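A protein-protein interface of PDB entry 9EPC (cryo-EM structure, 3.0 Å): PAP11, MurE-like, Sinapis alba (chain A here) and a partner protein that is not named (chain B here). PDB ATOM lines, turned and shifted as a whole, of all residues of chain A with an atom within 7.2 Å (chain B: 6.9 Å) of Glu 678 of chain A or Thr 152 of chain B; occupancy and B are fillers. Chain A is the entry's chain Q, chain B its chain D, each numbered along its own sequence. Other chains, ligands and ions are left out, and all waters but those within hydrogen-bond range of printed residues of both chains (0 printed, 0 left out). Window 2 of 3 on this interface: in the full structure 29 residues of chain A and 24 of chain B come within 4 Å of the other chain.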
ATOM      1  N   MET A 670      23.543 -27.238   0.589  1.00  0.00           N
ATOM      2  CA  MET A 670      23.160 -26.356  -0.506  1.00  0.00           C
ATOM      3  C   MET A 670      21.729 -26.624  -0.947  1.00  0.00           C
ATOM      4  O   MET A 670      20.977 -25.689  -1.243  1.00  0.00           O
ATOM      5  CB  MET A 670      24.124 -26.521  -1.679  1.00  0.00           C
ATOM      6  CG  MET A 670      23.724 -25.743  -2.917  1.00  0.00           C
ATOM      7  SD  MET A 670      23.760 -23.962  -2.661  1.00  0.00           S
ATOM      8  CE  MET A 670      25.516 -23.696  -2.465  1.00  0.00           C
ATOM      9  N   GLN A 671      21.330 -27.898  -0.983  1.00  0.00           N
ATOM     10  CA  GLN A 671      19.958 -28.233  -1.347  1.00  0.00           C
ATOM     11  C   GLN A 671      18.967 -27.625  -0.365  1.00  0.00           C
ATOM     12  O   GLN A 671      17.952 -27.048  -0.768  1.00  0.00           O
ATOM     13  CB  GLN A 671      19.787 -29.750  -1.409  1.00  0.00           C
ATOM     14  CG  GLN A 671      18.362 -30.193  -1.671  1.00  0.00           C
ATOM     15  CD  GLN A 671      18.195 -31.694  -1.583  1.00  0.00           C
ATOM     16  OE1 GLN A 671      19.153 -32.423  -1.328  1.00  0.00           O
ATOM     17  NE2 GLN A 671      16.972 -32.166  -1.793  1.00  0.00           N
ATOM     18  N   TYR A 673      19.417 -25.015   1.545  1.00  0.00           N
ATOM     19  CA  TYR A 673      19.427 -23.563   1.406  1.00  0.00           C
ATOM     20  C   TYR A 673      18.564 -23.117   0.235  1.00  0.00           C
ATOM     21  O   TYR A 673      17.815 -22.138   0.342  1.00  0.00           O
ATOM     22  CB  TYR A 673      20.859 -23.061   1.238  1.00  0.00           C
ATOM     23  CG  TYR A 673      20.959 -21.566   1.065  1.00  0.00           C
ATOM     24  CD1 TYR A 673      20.973 -20.722   2.164  1.00  0.00           C
ATOM     25  CD2 TYR A 673      21.042 -20.999  -0.198  1.00  0.00           C
ATOM     26  CE1 TYR A 673      21.064 -19.356   2.011  1.00  0.00           C
ATOM     27  CE2 TYR A 673      21.131 -19.632  -0.360  1.00  0.00           C
ATOM     28  CZ  TYR A 673      21.144 -18.817   0.748  1.00  0.00           C
ATOM     29  OH  TYR A 673      21.235 -17.455   0.590  1.00  0.00           O
ATOM     30  N   LEU A 674      18.654 -23.821  -0.894  1.00  0.00           N
ATOM     31  CA  LEU A 674      17.864 -23.443  -2.059  1.00  0.00           C
ATOM     32  C   LEU A 674      16.379 -23.693  -1.838  1.00  0.00           C
ATOM     33  O   LEU A 674      15.544 -22.995  -2.425  1.00  0.00           O
ATOM     34  CB  LEU A 674      18.358 -24.195  -3.291  1.00  0.00           C
ATOM     35  CG  LEU A 674      19.800 -23.869  -3.676  1.00  0.00           C
ATOM     36  CD1 LEU A 674      20.214 -24.638  -4.912  1.00  0.00           C
ATOM     37  CD2 LEU A 674      19.962 -22.376  -3.889  1.00  0.00           C
ATOM     38  N   LYS A 675      16.028 -24.676  -1.006  1.00  0.00           N
ATOM     39  CA  LYS A 675      14.622 -24.890  -0.682  1.00  0.00           C
ATOM     40  C   LYS A 675      14.038 -23.680   0.030  1.00  0.00           C
ATOM     41  O   LYS A 675      12.904 -23.274  -0.248  1.00  0.00           O
ATOM     42  CB  LYS A 675      14.460 -26.146   0.172  1.00  0.00           C
ATOM     43  CG  LYS A 675      14.786 -27.431  -0.561  1.00  0.00           C
ATOM     44  CD  LYS A 675      13.948 -27.574  -1.818  1.00  0.00           C
ATOM     45  CE  LYS A 675      14.360 -28.798  -2.619  1.00  0.00           C
ATOM     46  NZ  LYS A 675      14.208 -30.053  -1.835  1.00  0.00           N
ATOM     47  N   HIS A 676      14.798 -23.088   0.953  1.00  0.00           N
ATOM     48  CA  HIS A 676      14.358 -21.844   1.573  1.00  0.00           C
ATOM     49  C   HIS A 676      14.295 -20.714   0.559  1.00  0.00           C
ATOM     50  O   HIS A 676      13.477 -19.798   0.700  1.00  0.00           O
ATOM     51  CB  HIS A 676      15.285 -21.473   2.728  1.00  0.00           C
ATOM     52  CG  HIS A 676      15.277 -22.463   3.849  1.00  0.00           C
ATOM     53  ND1 HIS A 676      14.177 -22.666   4.653  1.00  0.00           N
ATOM     54  CD2 HIS A 676      16.235 -23.304   4.302  1.00  0.00           C
ATOM     55  CE1 HIS A 676      14.457 -23.590   5.553  1.00  0.00           C
ATOM     56  NE2 HIS A 676      15.700 -23.994   5.362  1.00  0.00           N
ATOM     57  N   GLY A 677      15.145 -20.760  -0.469  1.00  0.00           N
ATOM     58  CA  GLY A 677      15.084 -19.756  -1.515  1.00  0.00           C
ATOM     59  C   GLY A 677      13.772 -19.771  -2.270  1.00  0.00           C
ATOM     60  O   GLY A 677      13.297 -18.724  -2.718  1.00  0.00           O
ATOM     61  N   GLU A 678      13.171 -20.952  -2.426  1.00  0.00           N
ATOM     62  CA  GLU A 678      11.859 -21.035  -3.058  1.00  0.00           C
ATOM     63  C   GLU A 678      10.812 -20.288  -2.244  1.00  0.00           C
ATOM     64  O   GLU A 678       9.931 -19.628  -2.805  1.00  0.00           O
ATOM     65  CB  GLU A 678      11.452 -22.496  -3.235  1.00  0.00           C
ATOM     66  CG  GLU A 678      12.406 -23.309  -4.086  1.00  0.00           C
ATOM     67  CD  GLU A 678      11.968 -24.753  -4.234  1.00  0.00           C
ATOM     68  OE1 GLU A 678      10.946 -25.129  -3.623  1.00  0.00           O
ATOM     69  OE2 GLU A 678      12.644 -25.510  -4.960  1.00  0.00           O
ATOM     70  N   HIS A 679      10.894 -20.378  -0.920  1.00  0.00           N
ATOM     71  CA  HIS A 679       9.933 -19.726  -0.043  1.00  0.00           C
ATOM     72  C   HIS A 679      10.261 -18.261   0.206  1.00  0.00           C
ATOM     73  O   HIS A 679       9.507 -17.590   0.919  1.00  0.00           O
ATOM     74  CB  HIS A 679       9.854 -20.467   1.293  1.00  0.00           C
ATOM     75  CG  HIS A 679       9.591 -21.934   1.154  1.00  0.00           C
ATOM     76  ND1 HIS A 679       9.138 -22.500  -0.018  1.00  0.00           N
ATOM     77  CD2 HIS A 679       9.720 -22.950   2.037  1.00  0.00           C
ATOM     78  CE1 HIS A 679       8.998 -23.803   0.150  1.00  0.00           C
ATOM     79  NE2 HIS A 679       9.346 -24.102   1.389  1.00  0.00           N
ATOM     80  N   ASP A 680      11.361 -17.758  -0.358  1.00  0.00           N
ATOM     81  CA  ASP A 680      11.769 -16.362  -0.197  1.00  0.00           C
ATOM     82  C   ASP A 680      11.933 -16.001   1.277  1.00  0.00           C
ATOM     83  O   ASP A 680      11.579 -14.902   1.709  1.00  0.00           O
ATOM     84  CB  ASP A 680      10.785 -15.415  -0.884  1.00  0.00           C
ATOM     85  CG  ASP A 680      10.647 -15.694  -2.366  1.00  0.00           C
ATOM     86  OD1 ASP A 680      11.633 -16.150  -2.981  1.00  0.00           O
ATOM     87  OD2 ASP A 680       9.552 -15.455  -2.918  1.00  0.00           O
ATOM     88  N   TYR A 681      12.475 -16.934   2.055  1.00  0.00           N
ATOM     89  CA  TYR A 681      12.678 -16.706   3.483  1.00  0.00           C
ATOM     90  C   TYR A 681      13.774 -17.646   3.962  1.00  0.00           C
ATOM     91  O   TYR A 681      13.578 -18.864   3.979  1.00  0.00           O
ATOM     92  CB  TYR A 681      11.386 -16.929   4.257  1.00  0.00           C
ATOM     93  CG  TYR A 681      11.590 -17.100   5.744  1.00  0.00           C
ATOM     94  CD1 TYR A 681      11.868 -16.010   6.555  1.00  0.00           C
ATOM     95  CD2 TYR A 681      11.497 -18.352   6.335  1.00  0.00           C
ATOM     96  CE1 TYR A 681      12.052 -16.162   7.914  1.00  0.00           C
ATOM     97  CE2 TYR A 681      11.680 -18.514   7.692  1.00  0.00           C
ATOM     98  CZ  TYR A 681      11.958 -17.416   8.477  1.00  0.00           C
ATOM     99  OH  TYR A 681      12.140 -17.572   9.830  1.00  0.00           O
ATOM    100  N   TYR A 682      14.916 -17.081   4.349  1.00  0.00           N
ATOM    101  CA  TYR A 682      16.012 -17.868   4.889  1.00  0.00           C
ATOM    102  C   TYR A 682      15.952 -17.826   6.404  1.00  0.00           C
ATOM    103  O   TYR A 682      16.100 -16.740   6.988  1.00  0.00           O
ATOM    104  CB  TYR A 682      17.349 -17.335   4.394  1.00  0.00           C
ATOM    105  CG  TYR A 682      17.437 -17.259   2.890  1.00  0.00           C
ATOM    106  CD1 TYR A 682      17.676 -18.396   2.133  1.00  0.00           C
ATOM    107  CD2 TYR A 682      17.276 -16.053   2.226  1.00  0.00           C
ATOM    108  CE1 TYR A 682      17.756 -18.333   0.759  1.00  0.00           C
ATOM    109  CE2 TYR A 682      17.354 -15.981   0.851  1.00  0.00           C
ATOM    110  CZ  TYR A 682      17.594 -17.124   0.123  1.00  0.00           C
ATOM    111  OH  TYR A 682      17.673 -17.058  -1.248  1.00  0.00           O
ATOM    112  N   ARG B 149      12.476 -16.351 -11.432  1.00  0.00           N
ATOM    113  CA  ARG B 149      13.060 -17.576 -10.898  1.00  0.00           C
ATOM    114  C   ARG B 149      13.065 -18.722 -11.915  1.00  0.00           C
ATOM    115  O   ARG B 149      12.524 -19.799 -11.643  1.00  0.00           O
ATOM    116  CB  ARG B 149      12.339 -17.996  -9.625  1.00  0.00           C
ATOM    117  CG  ARG B 149      12.427 -16.991  -8.496  1.00  0.00           C
ATOM    118  CD  ARG B 149      13.826 -16.933  -7.916  1.00  0.00           C
ATOM    119  NE  ARG B 149      13.887 -16.054  -6.755  1.00  0.00           N
ATOM    120  CZ  ARG B 149      13.546 -16.418  -5.526  1.00  0.00           C
ATOM    121  NH1 ARG B 149      13.114 -17.640  -5.262  1.00  0.00           N
ATOM    122  NH2 ARG B 149      13.639 -15.533  -4.538  1.00  0.00           N
ATOM    123  N   PRO B 150      13.656 -18.522 -13.096  1.00  0.00           N
ATOM    124  CA  PRO B 150      13.731 -19.637 -14.052  1.00  0.00           C
ATOM    125  C   PRO B 150      14.550 -20.802 -13.531  1.00  0.00           C
ATOM    126  O   PRO B 150      14.250 -21.961 -13.843  1.00  0.00           O
ATOM    127  CB  PRO B 150      14.380 -18.998 -15.290  1.00  0.00           C
ATOM    128  CG  PRO B 150      14.296 -17.522 -15.067  1.00  0.00           C
ATOM    129  CD  PRO B 150      14.373 -17.340 -13.596  1.00  0.00           C
ATOM    130  N   ILE B 151      15.576 -20.521 -12.734  1.00  0.00           N
ATOM    131  CA  ILE B 151      16.506 -21.527 -12.240  1.00  0.00           C
ATOM    132  C   ILE B 151      16.387 -21.589 -10.726  1.00  0.00           C
ATOM    133  O   ILE B 151      16.451 -20.556 -10.050  1.00  0.00           O
ATOM    134  CB  ILE B 151      17.951 -21.210 -12.660  1.00  0.00           C
ATOM    135  CG1 ILE B 151      18.038 -21.021 -14.173  1.00  0.00           C
ATOM    136  CG2 ILE B 151      18.889 -22.313 -12.206  1.00  0.00           C
ATOM    137  CD1 ILE B 151      19.423 -20.660 -14.660  1.00  0.00           C
ATOM    138  N   THR B 152      16.213 -22.798 -10.196  1.00  0.00           N
ATOM    139  CA  THR B 152      16.172 -23.012  -8.759  1.00  0.00           C
ATOM    140  C   THR B 152      17.422 -23.689  -8.217  1.00  0.00           C
ATOM    141  O   THR B 152      17.699 -23.572  -7.021  1.00  0.00           O
ATOM    142  CB  THR B 152      14.943 -23.852  -8.382  1.00  0.00           C
ATOM    143  OG1 THR B 152      13.822 -23.429  -9.166  1.00  0.00           O
ATOM    144  CG2 THR B 152      14.605 -23.675  -6.915  1.00  0.00           C
ATOM    145  N   LYS B 153      18.187 -24.368  -9.062  1.00  0.00           N
ATOM    146  CA  LYS B 153      19.413 -25.037  -8.640  1.00  0.00           C
ATOM    147  C   LYS B 153      20.545 -24.073  -8.337  1.00  0.00           C
ATOM    148  O   LYS B 153      21.658 -24.537  -8.068  1.00  0.00           O
ATOM    149  CB  LYS B 153      19.861 -26.036  -9.708  1.00  0.00           C
ATOM    150  CG  LYS B 153      19.294 -27.439  -9.543  1.00  0.00           C
ATOM    151  CD  LYS B 153      17.795 -27.481  -9.777  1.00  0.00           C
ATOM    152  CE  LYS B 153      17.254 -28.890  -9.607  1.00  0.00           C
ATOM    153  NZ  LYS B 153      17.903 -29.849 -10.541  1.00  0.00           N
ATOM    154  N   LYS B 154      20.329 -22.763  -8.374  1.00  0.00           N
ATOM    155  CA  LYS B 154      21.361 -21.789  -8.063  1.00  0.00           C
ATOM    156  C   LYS B 154      20.775 -20.709  -7.169  1.00  0.00           C
ATOM    157  O   LYS B 154      19.571 -20.435  -7.233  1.00  0.00           O
ATOM    158  CB  LYS B 154      21.942 -21.158  -9.338  1.00  0.00           C
ATOM    159  CG  LYS B 154      22.740 -22.125 -10.192  1.00  0.00           C
ATOM    160  CD  LYS B 154      23.361 -21.424 -11.385  1.00  0.00           C
ATOM    161  CE  LYS B 154      24.270 -22.360 -12.159  1.00  0.00           C
ATOM    162  NZ  LYS B 154      23.543 -23.570 -12.630  1.00  0.00           N
ATOM    163  N   PRO B 155      21.594 -20.091  -6.317  1.00  0.00           N
ATOM    164  CA  PRO B 155      21.070 -19.075  -5.397  1.00  0.00           C
ATOM    165  C   PRO B 155      20.507 -17.872  -6.138  1.00  0.00           C
ATOM    166  O   PRO B 155      21.042 -17.439  -7.160  1.00  0.00           O
ATOM    167  CB  PRO B 155      22.295 -18.693  -4.560  1.00  0.00           C
ATOM    168  CG  PRO B 155      23.221 -19.850  -4.688  1.00  0.00           C
ATOM    169  CD  PRO B 155      23.017 -20.373  -6.071  1.00  0.00           C
ATOM    170  N   THR B 156      19.416 -17.328  -5.602  1.00  0.00           N
ATOM    171  CA  THR B 156      18.773 -16.145  -6.154  1.00  0.00           C
ATOM    172  C   THR B 156      18.408 -15.203  -5.017  1.00  0.00           C
ATOM    173  O   THR B 156      18.103 -15.642  -3.905  1.00  0.00           O
ATOM    174  CB  THR B 156      17.512 -16.496  -6.957  1.00  0.00           C
ATOM    175  OG1 THR B 156      16.618 -17.260  -6.140  1.00  0.00           O
ATOM    176  CG2 THR B 156      17.869 -17.297  -8.200  1.00  0.00           C
ATOM    177  N   ARG B 161       8.312 -13.711  -8.396  1.00  0.00           N
ATOM    178  CA  ARG B 161       7.681 -15.019  -8.269  1.00  0.00           C
ATOM    179  C   ARG B 161       7.579 -15.766  -9.593  1.00  0.00           C
ATOM    180  O   ARG B 161       8.087 -16.884  -9.706  1.00  0.00           O
ATOM    181  CB  ARG B 161       6.290 -14.863  -7.641  1.00  0.00           C
ATOM    182  CG  ARG B 161       5.537 -16.171  -7.483  1.00  0.00           C
ATOM    183  CD  ARG B 161       6.349 -17.175  -6.683  1.00  0.00           C
ATOM    184  NE  ARG B 161       6.664 -16.681  -5.348  1.00  0.00           N
ATOM    185  CZ  ARG B 161       7.412 -17.332  -4.468  1.00  0.00           C
ATOM    186  NH1 ARG B 161       7.947 -18.509  -4.751  1.00  0.00           N
ATOM    187  NH2 ARG B 161       7.630 -16.789  -3.274  1.00  0.00           N
ATOM    188  N   ARG B 190      19.595 -15.884 -14.377  1.00  0.00           N
ATOM    189  CA  ARG B 190      19.263 -16.632 -13.173  1.00  0.00           C
ATOM    190  C   ARG B 190      18.052 -16.055 -12.454  1.00  0.00           C
ATOM    191  O   ARG B 190      17.373 -16.785 -11.726  1.00  0.00           O
ATOM    192  CB  ARG B 190      20.469 -16.659 -12.234  1.00  0.00           C
ATOM    193  CG  ARG B 190      20.375 -17.679 -11.122  1.00  0.00           C
ATOM    194  CD  ARG B 190      21.653 -17.700 -10.309  1.00  0.00           C
ATOM    195  NE  ARG B 190      22.824 -17.892 -11.153  1.00  0.00           N
ATOM    196  CZ  ARG B 190      24.059 -18.040 -10.695  1.00  0.00           C
ATOM    197  NH1 ARG B 190      24.320 -18.035  -9.398  1.00  0.00           N
ATOM    198  NH2 ARG B 190      25.057 -18.198 -11.559  1.00  0.00           N
ATOM    199  N   GLU B 201      15.587 -23.252 -19.772  1.00  0.00           N
ATOM    200  CA  GLU B 201      16.224 -23.304 -18.461  1.00  0.00           C
ATOM    201  C   GLU B 201      15.270 -23.856 -17.413  1.00  0.00           C
ATOM    202  O   GLU B 201      15.677 -24.625 -16.535  1.00  0.00           O
ATOM    203  CB  GLU B 201      16.723 -21.916 -18.062  1.00  0.00           C
ATOM    204  CG  GLU B 201      17.758 -21.339 -19.010  1.00  0.00           C
ATOM    205  CD  GLU B 201      18.988 -22.215 -19.136  1.00  0.00           C
ATOM    206  OE1 GLU B 201      19.377 -22.849 -18.134  1.00  0.00           O
ATOM    207  OE2 GLU B 201      19.567 -22.271 -20.241  1.00  0.00           O
ATOM    208  N   ASP B 205      15.895 -27.111 -15.179  1.00  0.00           N
ATOM    209  CA  ASP B 205      15.841 -27.015 -13.727  1.00  0.00           C
ATOM    210  C   ASP B 205      14.833 -27.972 -13.107  1.00  0.00           C
ATOM    211  O   ASP B 205      14.899 -28.211 -11.897  1.00  0.00           O
ATOM    212  CB  ASP B 205      15.517 -25.572 -13.333  1.00  0.00           C
ATOM    213  CG  ASP B 205      15.676 -25.314 -11.851  1.00  0.00           C
ATOM    214  OD1 ASP B 205      14.769 -25.678 -11.075  1.00  0.00           O
ATOM    215  OD2 ASP B 205      16.714 -24.743 -11.458  1.00  0.00           O
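The guanidinium group of Arg 149 of chain B is in hydrogen-bond range of the backbone carbonyl oxygen of Gly 677 of chain A (2.8 Å).
NH1 of Arg 161 of chain B sits at hydrogen-bond distance from O of Glu 678 of chain A (3.0 Å).
OD1 of Asp 680 of chain A lies within salt-bridge range of NH2 of Arg 149 of chain B (2.6 Å).
NH1 of Arg 161 of chain B is in salt-bridge range of OD2 of Asp 680 of chain A (3.9 Å).
The backbone carbonyl oxygen (O) of Thr 156 of chain B is in hydrogen-bond range of the side-chain hydroxyl (OH) of Tyr 682 of chain A (3.0 Å).
Tyr 673 of chain A touches none of the printed residues of chain B.
Printed residues of chain B within 4 Å of Leu 674 of chain A: Thr 152, Lys 153, Lys 154 and Pro 155.
Glu 678 of chain A touches just these residues of chain B: Thr 152 and Arg 161.
Printed residues of chain B within 4 Å of Asp 680 of chain A: Arg 149 and Arg 161.
Printed residues of chain B within 4 Å of Tyr 682 of chain A: Thr 156 (3.0 Å).
Of the printed residues of chain A, Thr 152 of chain B touches Leu 674 and Glu 678.
Of the printed residues of chain A, Pro 155 of chain B touches Leu 674 (3.7 Å).
Asp 205 of chain B touches none of the printed residues of chain A.
The nearest printed residue of chain A that does not touch Arg 149 of chain B is Glu 678 of chain A (4.2 Å).
Among the printed residues, merely in contact across the chains: Glu 678 of chain A with Thr 152 of chain B, Leu 674 of chain A with Thr 152 of chain B, Leu 674 of chain A with Lys 153 of chain B, Leu 674 of chain A with Pro 155 of chain B and Leu 674 of chain A with Lys 154 of chain B.
OG1 of Thr 156 of chain B sits at hydrogen-bond distance from NE of Arg 149 of chain B, 3.0 Å away.
OG1 of Thr 152 of chain B lies within hydrogen-bond range of OD1 of Asp 205 of chain B (3.1 Å).
The side-chain carboxylate (OD2) of Asp 205 of chain B lies within hydrogen-bond range of the backbone NH (N) of Lys 153 of chain B (2.8 Å).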
